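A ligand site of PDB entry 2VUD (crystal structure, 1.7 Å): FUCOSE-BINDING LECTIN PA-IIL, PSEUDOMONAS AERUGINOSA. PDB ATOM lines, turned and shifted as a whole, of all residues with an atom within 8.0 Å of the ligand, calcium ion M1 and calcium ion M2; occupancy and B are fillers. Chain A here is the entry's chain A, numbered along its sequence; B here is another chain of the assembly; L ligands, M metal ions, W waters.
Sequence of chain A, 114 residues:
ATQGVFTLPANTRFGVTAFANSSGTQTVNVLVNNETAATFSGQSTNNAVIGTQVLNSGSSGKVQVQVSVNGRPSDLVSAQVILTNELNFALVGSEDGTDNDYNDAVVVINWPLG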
ATOM      1  N   ALA A  20     -21.704 -20.158  21.647  1.00  0.00           N
ATOM      2  CA  ALA A  20     -22.660 -21.120  22.245  1.00  0.00           C
ATOM      3  C   ALA A  20     -24.123 -20.707  22.033  1.00  0.00           C
ATOM      4  O   ALA A  20     -24.482 -19.520  22.231  1.00  0.00           O
ATOM      5  CB  ALA A  20     -22.380 -21.290  23.755  1.00  0.00           C
ATOM      6  N   ASN A  21     -24.965 -21.684  21.674  1.00  0.00           N
ATOM      7  CA  ASN A  21     -26.403 -21.461  21.471  1.00  0.00           C
ATOM      8  C   ASN A  21     -27.222 -22.676  21.967  1.00  0.00           C
ATOM      9  O   ASN A  21     -27.849 -23.380  21.153  1.00  0.00           O
ATOM     10  CB  ASN A  21     -26.700 -21.175  20.006  1.00  0.00           C
ATOM     11  CG  ASN A  21     -26.210 -19.790  19.568  1.00  0.00           C
ATOM     12  OD1 ASN A  21     -26.806 -18.769  19.904  1.00  0.00           O
ATOM     13  ND2 ASN A  21     -25.091 -19.790  18.839  1.00  0.00           N
ATOM     14  N   SER A  22     -27.196 -22.911  23.274  1.00  0.00           N
ATOM     15  CA  SER A  22     -27.838 -24.119  23.832  1.00  0.00           C
ATOM     16  C   SER A  22     -28.117 -23.969  25.351  1.00  0.00           C
ATOM     17  O   SER A  22     -27.490 -23.147  26.027  1.00  0.00           O
ATOM     18  CB  SER A  22     -26.947 -25.363  23.604  1.00  0.00           C
ATOM     19  OG  SER A  22     -27.517 -26.553  24.162  1.00  0.00           O
ATOM     20  N   SER A  23     -29.057 -24.772  25.852  1.00  0.00           N
ATOM     21  CA  SER A  23     -29.286 -24.874  27.296  1.00  0.00           C
ATOM     22  C   SER A  23     -28.095 -25.499  28.013  1.00  0.00           C
ATOM     23  O   SER A  23     -27.836 -25.211  29.193  1.00  0.00           O
ATOM     24  CB  SER A  23     -30.562 -25.669  27.608  1.00  0.00           C
ATOM     25  OG  SER A  23     -30.474 -26.995  27.114  1.00  0.00           O
ATOM     26  N   GLY A  24     -27.372 -26.369  27.321  1.00  0.00           N
ATOM     27  CA  GLY A  24     -26.271 -27.116  27.959  1.00  0.00           C
ATOM     28  C   GLY A  24     -24.906 -26.450  27.824  1.00  0.00           C
ATOM     29  O   GLY A  24     -24.629 -25.724  26.864  1.00  0.00           O
ATOM     30  N   GLN A  26     -21.181 -26.091  26.830  1.00  0.00           N
ATOM     31  CA  GLN A  26     -20.374 -26.609  25.712  1.00  0.00           C
ATOM     32  C   GLN A  26     -18.899 -26.690  26.108  1.00  0.00           C
ATOM     33  O   GLN A  26     -18.363 -25.771  26.748  1.00  0.00           O
ATOM     34  CB  GLN A  26     -20.503 -25.657  24.494  1.00  0.00           C
ATOM     35  CG  GLN A  26     -21.949 -25.314  24.096  1.00  0.00           C
ATOM     36  CD  GLN A  26     -22.682 -26.515  23.489  1.00  0.00           C
ATOM     37  OE1 GLN A  26     -22.201 -27.091  22.518  1.00  0.00           O
ATOM     38  NE2 GLN A  26     -23.868 -26.871  24.051  1.00  0.00           N
ATOM     39  N   GLN A  43     -21.708 -21.458  28.667  1.00  0.00           N
ATOM     40  CA  GLN A  43     -23.128 -21.663  28.365  1.00  0.00           C
ATOM     41  C   GLN A  43     -23.828 -20.368  27.977  1.00  0.00           C
ATOM     42  O   GLN A  43     -23.707 -19.354  28.663  1.00  0.00           O
ATOM     43  CB  GLN A  43     -23.875 -22.282  29.574  1.00  0.00           C
ATOM     44  CG  GLN A  43     -25.311 -22.752  29.248  1.00  0.00           C
ATOM     45  CD  GLN A  43     -26.358 -21.628  29.352  1.00  0.00           C
ATOM     46  OE1 GLN A  43     -26.258 -20.768  30.227  1.00  0.00           O
ATOM     47  NE2 GLN A  43     -27.364 -21.652  28.470  1.00  0.00           N
ATOM     48  N   SER A  44     -24.594 -20.412  26.869  1.00  0.00           N
ATOM     49  CA  SER A  44     -25.360 -19.263  26.394  1.00  0.00           C
ATOM     50  C   SER A  44     -26.412 -19.722  25.404  1.00  0.00           C
ATOM     51  O   SER A  44     -26.188 -20.672  24.631  1.00  0.00           O
ATOM     52  CB  SER A  44     -24.428 -18.188  25.777  1.00  0.00           C
ATOM     53  OG  SER A  44     -25.181 -17.066  25.297  1.00  0.00           O
ATOM     54  N   THR A  45     -27.557 -19.042  25.401  1.00  0.00           N
ATOM     55  CA  THR A  45     -28.520 -19.195  24.316  1.00  0.00           C
ATOM     56  C   THR A  45     -28.587 -17.932  23.458  1.00  0.00           C
ATOM     57  O   THR A  45     -29.545 -17.730  22.715  1.00  0.00           O
ATOM     58  CB  THR A  45     -29.948 -19.534  24.859  1.00  0.00           C
ATOM     59  OG1 THR A  45     -30.318 -18.571  25.850  1.00  0.00           O
ATOM     60  CG2 THR A  45     -29.978 -20.928  25.440  1.00  0.00           C
ATOM     61  N   VAL A  69     -20.925 -32.145  25.101  1.00  0.00           N
ATOM     62  CA  VAL A  69     -22.026 -31.546  25.899  1.00  0.00           C
ATOM     63  C   VAL A  69     -22.703 -32.629  26.747  1.00  0.00           C
ATOM     64  O   VAL A  69     -22.991 -33.722  26.230  1.00  0.00           O
ATOM     65  CB  VAL A  69     -23.086 -30.840  25.031  1.00  0.00           C
ATOM     66  CG1 VAL A  69     -24.145 -30.102  25.872  1.00  0.00           C
ATOM     67  CG2 VAL A  69     -22.456 -29.875  24.039  1.00  0.00           C
ATOM     68  N   SER A  94     -22.203 -27.849  15.429  1.00  0.00           N
ATOM     69  CA  SER A  94     -22.385 -29.038  16.243  1.00  0.00           C
ATOM     70  C   SER A  94     -23.782 -29.124  16.820  1.00  0.00           C
ATOM     71  O   SER A  94     -24.393 -28.090  17.147  1.00  0.00           O
ATOM     72  CB  SER A  94     -21.355 -29.065  17.376  1.00  0.00           C
ATOM     73  OG  SER A  94     -21.504 -27.946  18.241  1.00  0.00           O
ATOM     74  N   GLU A  95     -24.260 -30.365  16.969  1.00  0.00           N
ATOM     75  CA  GLU A  95     -25.593 -30.628  17.551  1.00  0.00           C
ATOM     76  C   GLU A  95     -25.506 -31.503  18.814  1.00  0.00           C
ATOM     77  O   GLU A  95     -24.931 -32.615  18.801  1.00  0.00           O
ATOM     78  CB  GLU A  95     -26.481 -31.316  16.487  1.00  0.00           C
ATOM     79  CG  GLU A  95     -27.852 -31.692  16.959  1.00  0.00           C
ATOM     80  CD  GLU A  95     -28.677 -30.451  17.359  1.00  0.00           C
ATOM     81  OE1 GLU A  95     -28.630 -29.452  16.621  1.00  0.00           O
ATOM     82  OE2 GLU A  95     -29.330 -30.488  18.435  1.00  0.00           O
ATOM     83  N   ASP A  96     -26.096 -31.022  19.891  1.00  0.00           N
ATOM     84  CA  ASP A  96     -26.054 -31.746  21.158  1.00  0.00           C
ATOM     85  C   ASP A  96     -27.379 -32.401  21.526  1.00  0.00           C
ATOM     86  O   ASP A  96     -27.436 -33.167  22.489  1.00  0.00           O
ATOM     87  CB  ASP A  96     -25.568 -30.813  22.290  1.00  0.00           C
ATOM     88  CG  ASP A  96     -26.504 -29.647  22.531  1.00  0.00           C
ATOM     89  OD1 ASP A  96     -27.703 -29.740  22.213  1.00  0.00           O
ATOM     90  OD2 ASP A  96     -26.046 -28.637  23.139  1.00  0.00           O
ATOM     91  N   GLY A  97     -28.434 -32.110  20.757  1.00  0.00           N
ATOM     92  CA  GLY A  97     -29.777 -32.545  21.114  1.00  0.00           C
ATOM     93  C   GLY A  97     -30.500 -33.180  19.932  1.00  0.00           C
ATOM     94  O   GLY A  97     -29.934 -33.974  19.181  1.00  0.00           O
ATOM     95  N   THR A  98     -31.769 -32.800  19.776  1.00  0.00           N
ATOM     96  CA  THR A  98     -32.662 -33.454  18.818  1.00  0.00           C
ATOM     97  C   THR A  98     -33.229 -32.499  17.762  1.00  0.00           C
ATOM     98  O   THR A  98     -33.833 -32.945  16.785  1.00  0.00           O
ATOM     99  CB  THR A  98     -33.840 -34.123  19.577  1.00  0.00           C
ATOM    100  OG1 THR A  98     -34.467 -33.158  20.427  1.00  0.00           O
ATOM    101  CG2 THR A  98     -33.336 -35.283  20.462  1.00  0.00           C
ATOM    102  N   ASP A  99     -33.028 -31.187  17.949  1.00  0.00           N
ATOM    103  CA  ASP A  99     -33.704 -30.219  17.092  1.00  0.00           C
ATOM    104  C   ASP A  99     -32.958 -29.964  15.754  1.00  0.00           C
ATOM    105  O   ASP A  99     -33.533 -29.372  14.847  1.00  0.00           O
ATOM    106  CB  ASP A  99     -33.984 -28.881  17.826  1.00  0.00           C
ATOM    107  CG  ASP A  99     -32.728 -28.095  18.188  1.00  0.00           C
ATOM    108  OD1 ASP A  99     -31.626 -28.703  18.296  1.00  0.00           O
ATOM    109  OD2 ASP A  99     -32.839 -26.876  18.346  1.00  0.00           O
ATOM    110  N   ASN A 100     -31.717 -30.444  15.664  1.00  0.00           N
ATOM    111  CA  ASN A 100     -30.878 -30.320  14.449  1.00  0.00           C
ATOM    112  C   ASN A 100     -30.678 -28.912  13.911  1.00  0.00           C
ATOM    113  O   ASN A 100     -30.650 -28.698  12.697  1.00  0.00           O
ATOM    114  CB  ASN A 100     -31.390 -31.245  13.341  1.00  0.00           C
ATOM    115  CG  ASN A 100     -31.278 -32.697  13.734  1.00  0.00           C
ATOM    116  OD1 ASN A 100     -30.406 -33.061  14.559  1.00  0.00           O
ATOM    117  ND2 ASN A 100     -32.120 -33.542  13.141  1.00  0.00           N
ATOM    118  N   ASP A 101     -30.521 -27.960  14.815  1.00  0.00           N
ATOM    119  CA  ASP A 101     -30.157 -26.593  14.371  1.00  0.00           C
ATOM    120  C   ASP A 101     -28.629 -26.435  14.148  1.00  0.00           C
ATOM    121  O   ASP A 101     -28.196 -25.533  13.440  1.00  0.00           O
ATOM    122  CB  ASP A 101     -30.725 -25.504  15.302  1.00  0.00           C
ATOM    123  CG  ASP A 101     -30.265 -25.637  16.763  1.00  0.00           C
ATOM    124  OD1 ASP A 101     -29.523 -26.606  17.087  1.00  0.00           O
ATOM    125  OD2 ASP A 101     -30.639 -24.740  17.567  1.00  0.00           O
ATOM    126  N   TYR A 102     -27.830 -27.317  14.767  1.00  0.00           N
ATOM    127  CA  TYR A 102     -26.377 -27.393  14.554  1.00  0.00           C
ATOM    128  C   TYR A 102     -25.580 -26.132  14.957  1.00  0.00           C
ATOM    129  O   TYR A 102     -24.470 -25.916  14.482  1.00  0.00           O
ATOM    130  CB  TYR A 102     -25.982 -27.927  13.129  1.00  0.00           C
ATOM    131  CG  TYR A 102     -26.103 -29.443  13.053  1.00  0.00           C
ATOM    132  CD1 TYR A 102     -25.000 -30.283  13.309  1.00  0.00           C
ATOM    133  CD2 TYR A 102     -27.337 -30.046  12.792  1.00  0.00           C
ATOM    134  CE1 TYR A 102     -25.128 -31.689  13.268  1.00  0.00           C
ATOM    135  CE2 TYR A 102     -27.472 -31.439  12.768  1.00  0.00           C
ATOM    136  CZ  TYR A 102     -26.362 -32.241  13.001  1.00  0.00           C
ATOM    137  OH  TYR A 102     -26.490 -33.619  12.975  1.00  0.00           O
ATOM    138  N   ASN A 103     -26.166 -25.315  15.857  1.00  0.00           N
ATOM    139  CA  ASN A 103     -25.547 -24.032  16.280  1.00  0.00           C
ATOM    140  C   ASN A 103     -25.118 -24.091  17.745  1.00  0.00           C
ATOM    141  O   ASN A 103     -24.624 -23.107  18.290  1.00  0.00           O
ATOM    142  CB  ASN A 103     -26.501 -22.844  16.074  1.00  0.00           C
ATOM    143  CG  ASN A 103     -27.705 -22.872  17.022  1.00  0.00           C
ATOM    144  OD1 ASN A 103     -27.859 -23.805  17.826  1.00  0.00           O
ATOM    145  ND2 ASN A 103     -28.548 -21.815  16.963  1.00  0.00           N
ATOM    146  N   ASP A 104     -25.329 -25.250  18.383  1.00  0.00           N
ATOM    147  CA  ASP A 104     -25.162 -25.374  19.826  1.00  0.00           C
ATOM    148  C   ASP A 104     -23.761 -24.961  20.281  1.00  0.00           C
ATOM    149  O   ASP A 104     -23.604 -24.299  21.333  1.00  0.00           O
ATOM    150  CB  ASP A 104     -25.489 -26.813  20.248  1.00  0.00           C
ATOM    151  CG  ASP A 104     -26.929 -27.184  19.926  1.00  0.00           C
ATOM    152  OD1 ASP A 104     -27.835 -26.279  20.061  1.00  0.00           O
ATOM    153  OD2 ASP A 104     -27.207 -28.363  19.530  1.00  0.00           O
ATOM    154  N   ALA A 105     -22.759 -25.359  19.475  1.00  0.00           N
ATOM    155  CA  ALA A 105     -21.421 -24.725  19.511  1.00  0.00           C
ATOM    156  C   ALA A 105     -20.946 -24.473  18.081  1.00  0.00           C
ATOM    157  O   ALA A 105     -20.833 -25.407  17.270  1.00  0.00           O
ATOM    158  CB  ALA A 105     -20.420 -25.620  20.222  1.00  0.00           C
ATOM    159  N   PRO B 112     -29.197 -19.525  12.376  1.00  0.00           N
ATOM    160  CA  PRO B 112     -29.941 -18.911  13.476  1.00  0.00           C
ATOM    161  C   PRO B 112     -29.279 -19.094  14.842  1.00  0.00           C
ATOM    162  O   PRO B 112     -28.319 -19.854  14.990  1.00  0.00           O
ATOM    163  CB  PRO B 112     -31.277 -19.661  13.452  1.00  0.00           C
ATOM    164  CG  PRO B 112     -30.929 -21.005  12.934  1.00  0.00           C
ATOM    165  CD  PRO B 112     -29.711 -20.872  12.051  1.00  0.00           C
ATOM    166  N   LEU B 113     -29.761 -18.348  15.832  1.00  0.00           N
ATOM    167  CA  LEU B 113     -29.238 -18.421  17.185  1.00  0.00           C
ATOM    168  C   LEU B 113     -30.241 -19.120  18.111  1.00  0.00           C
ATOM    169  O   LEU B 113     -31.358 -19.544  17.676  1.00  0.00           O
ATOM    170  CB  LEU B 113     -28.963 -17.023  17.722  1.00  0.00           C
ATOM    171  CG  LEU B 113     -28.186 -16.044  16.832  1.00  0.00           C
ATOM    172  CD1 LEU B 113     -28.030 -14.705  17.635  1.00  0.00           C
ATOM    173  CD2 LEU B 113     -26.811 -16.610  16.415  1.00  0.00           C
ATOM    174  N   GLY B 114     -29.853 -19.243  19.379  1.00  0.00           N
ATOM    175  CA  GLY B 114     -30.703 -19.835  20.414  1.00  0.00           C
ATOM    176  C   GLY B 114     -30.642 -21.340  20.548  1.00  0.00           C
ATOM    177  O   GLY B 114     -30.170 -22.058  19.643  1.00  0.00           O
ATOM    178  OXT GLY B 114     -31.116 -21.869  21.561  1.00  0.00           O
HETATM  179  C1  LIG L   1     -30.642 -27.504  23.545  1.00  0.00           C
HETATM  180  C2  LIG L   1     -30.232 -27.365  22.052  1.00  0.00           C
HETATM  181  C3  LIG L   1     -31.263 -26.540  21.275  1.00  0.00           C
HETATM  182  C4  LIG L   1     -31.653 -25.259  21.998  1.00  0.00           C
HETATM  183  C5  LIG L   1     -31.991 -25.482  23.503  1.00  0.00           C
HETATM  184  C6  LIG L   1     -32.222 -24.127  24.200  1.00  0.00           C
HETATM  185  O1  LIG L   1     -31.791 -28.310  23.682  1.00  0.00           O
HETATM  186  O2  LIG L   1     -30.116 -28.643  21.439  1.00  0.00           O
HETATM  187  O3  LIG L   1     -30.728 -26.245  19.961  1.00  0.00           O
HETATM  188  O4  LIG L   1     -30.590 -24.352  21.876  1.00  0.00           O
HETATM  189  O5  LIG L   1     -30.930 -26.226  24.117  1.00  0.00           O
HETATM  190 CA    CA M   1     -29.217 -24.468  19.600  1.00  0.00          CA
HETATM  191 CA    CA M   2     -29.422 -28.171  18.802  1.00  0.00          CA
HETATM  192  O   HOH W   1     -32.354 -30.478  21.346  1.00  0.00           O
HETATM  193  O   HOH W   2     -31.989 -29.085  26.249  1.00  0.00           O
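OG of Ser 22 lies within hydrogen-bond range of N of Gly 24, at 3.2 Å.
The backbone carbonyl oxygen of Asp 104 sits close to the side-chain amide oxygen of Gln 26, 3.3 Å away.
N of Asp 104 lies within hydrogen-bond range of O of Ser 94.
The backbone carbonyl oxygen (O) of Ser 44 sits at hydrogen-bond distance from the backbone NH (N) of Ser 22 (2.8 Å).
N of Tyr 102 sits close to OE1 of Glu 95 (2.9 Å).
OD2 of Asp 104 lies close to N of Asp 96 (2.9 Å).
The side-chain carboxylate of Glu 95 sits close to the backbone NH of Gly 97, at 3.0 Å.
The backbone carbonyl oxygen (O) of Ser 22 sits at hydrogen-bond distance from the side-chain amide nitrogen (NE2) of Gln 43 (2.9 Å).
The side-chain hydroxyl (OG) of Ser 23 lies within hydrogen-bond range of an oxygen (O5) of the ligand, at 3.1 Å.
An oxygen (O5) of the ligand lies close to the side-chain hydroxyl of Ser 22.
An oxygen (O2) of the ligand lies close to the side-chain carboxylate of Asp 96 (2.8 Å).
An oxygen (O5) of the ligand sits at hydrogen-bond distance from the backbone NH (N) of Ser 23 (2.9 Å).
Water W2 bridges O1 of the ligand and OG of Ser 23.
Water W1 bridges N of Thr 98 and O1 of the ligand.
Calcium ion M2 is bound by OD1 of Asp 99, 2.3 Å away.
Calcium ion M2 is bound by OD1 of Asp 101, 2.3 Å away.
OD2 of Asp 104 binds calcium ion M2 (2.3 Å).
Calcium ion M2 is bound by OE2 of Glu 95 (2.3 Å).
An oxygen (O3) of the ligand binds calcium ion M2 (2.6 Å).
Calcium ion M2 is bound by OE1 of Glu 95 (2.7 Å).
Calcium ion M2 is bound by an oxygen (O2) of the ligand, at 2.8 Å.
OD1 of Asp 104 is bound to calcium ion M2, 2.8 Å away.
Calcium ion M2 has eight donor atoms within binding distance.
Gly 97 touches the ligand.
Of the 25 residues printed, 10 come within 4 Å of the ligand.
Along chain A the residues within 4 Å of the ligand span positions 21 to 104.
Calcium ion M1 is bound by OD1 of Asp 104, OD1 of Asn 103, O of Asn 21, O3 of the ligand, OD2 of Asp 101, O of Gly 114 of chain B and O4 of the ligand.
Of the 25 residues printed, 5 come within 4 Å of calcium ion M1.
The nearest printed residue that does not touch calcium ion M1 is Ser 22 (4.5 Å).
The nearest printed residue that does not touch calcium ion M2 is Asp 96 (4.1 Å).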
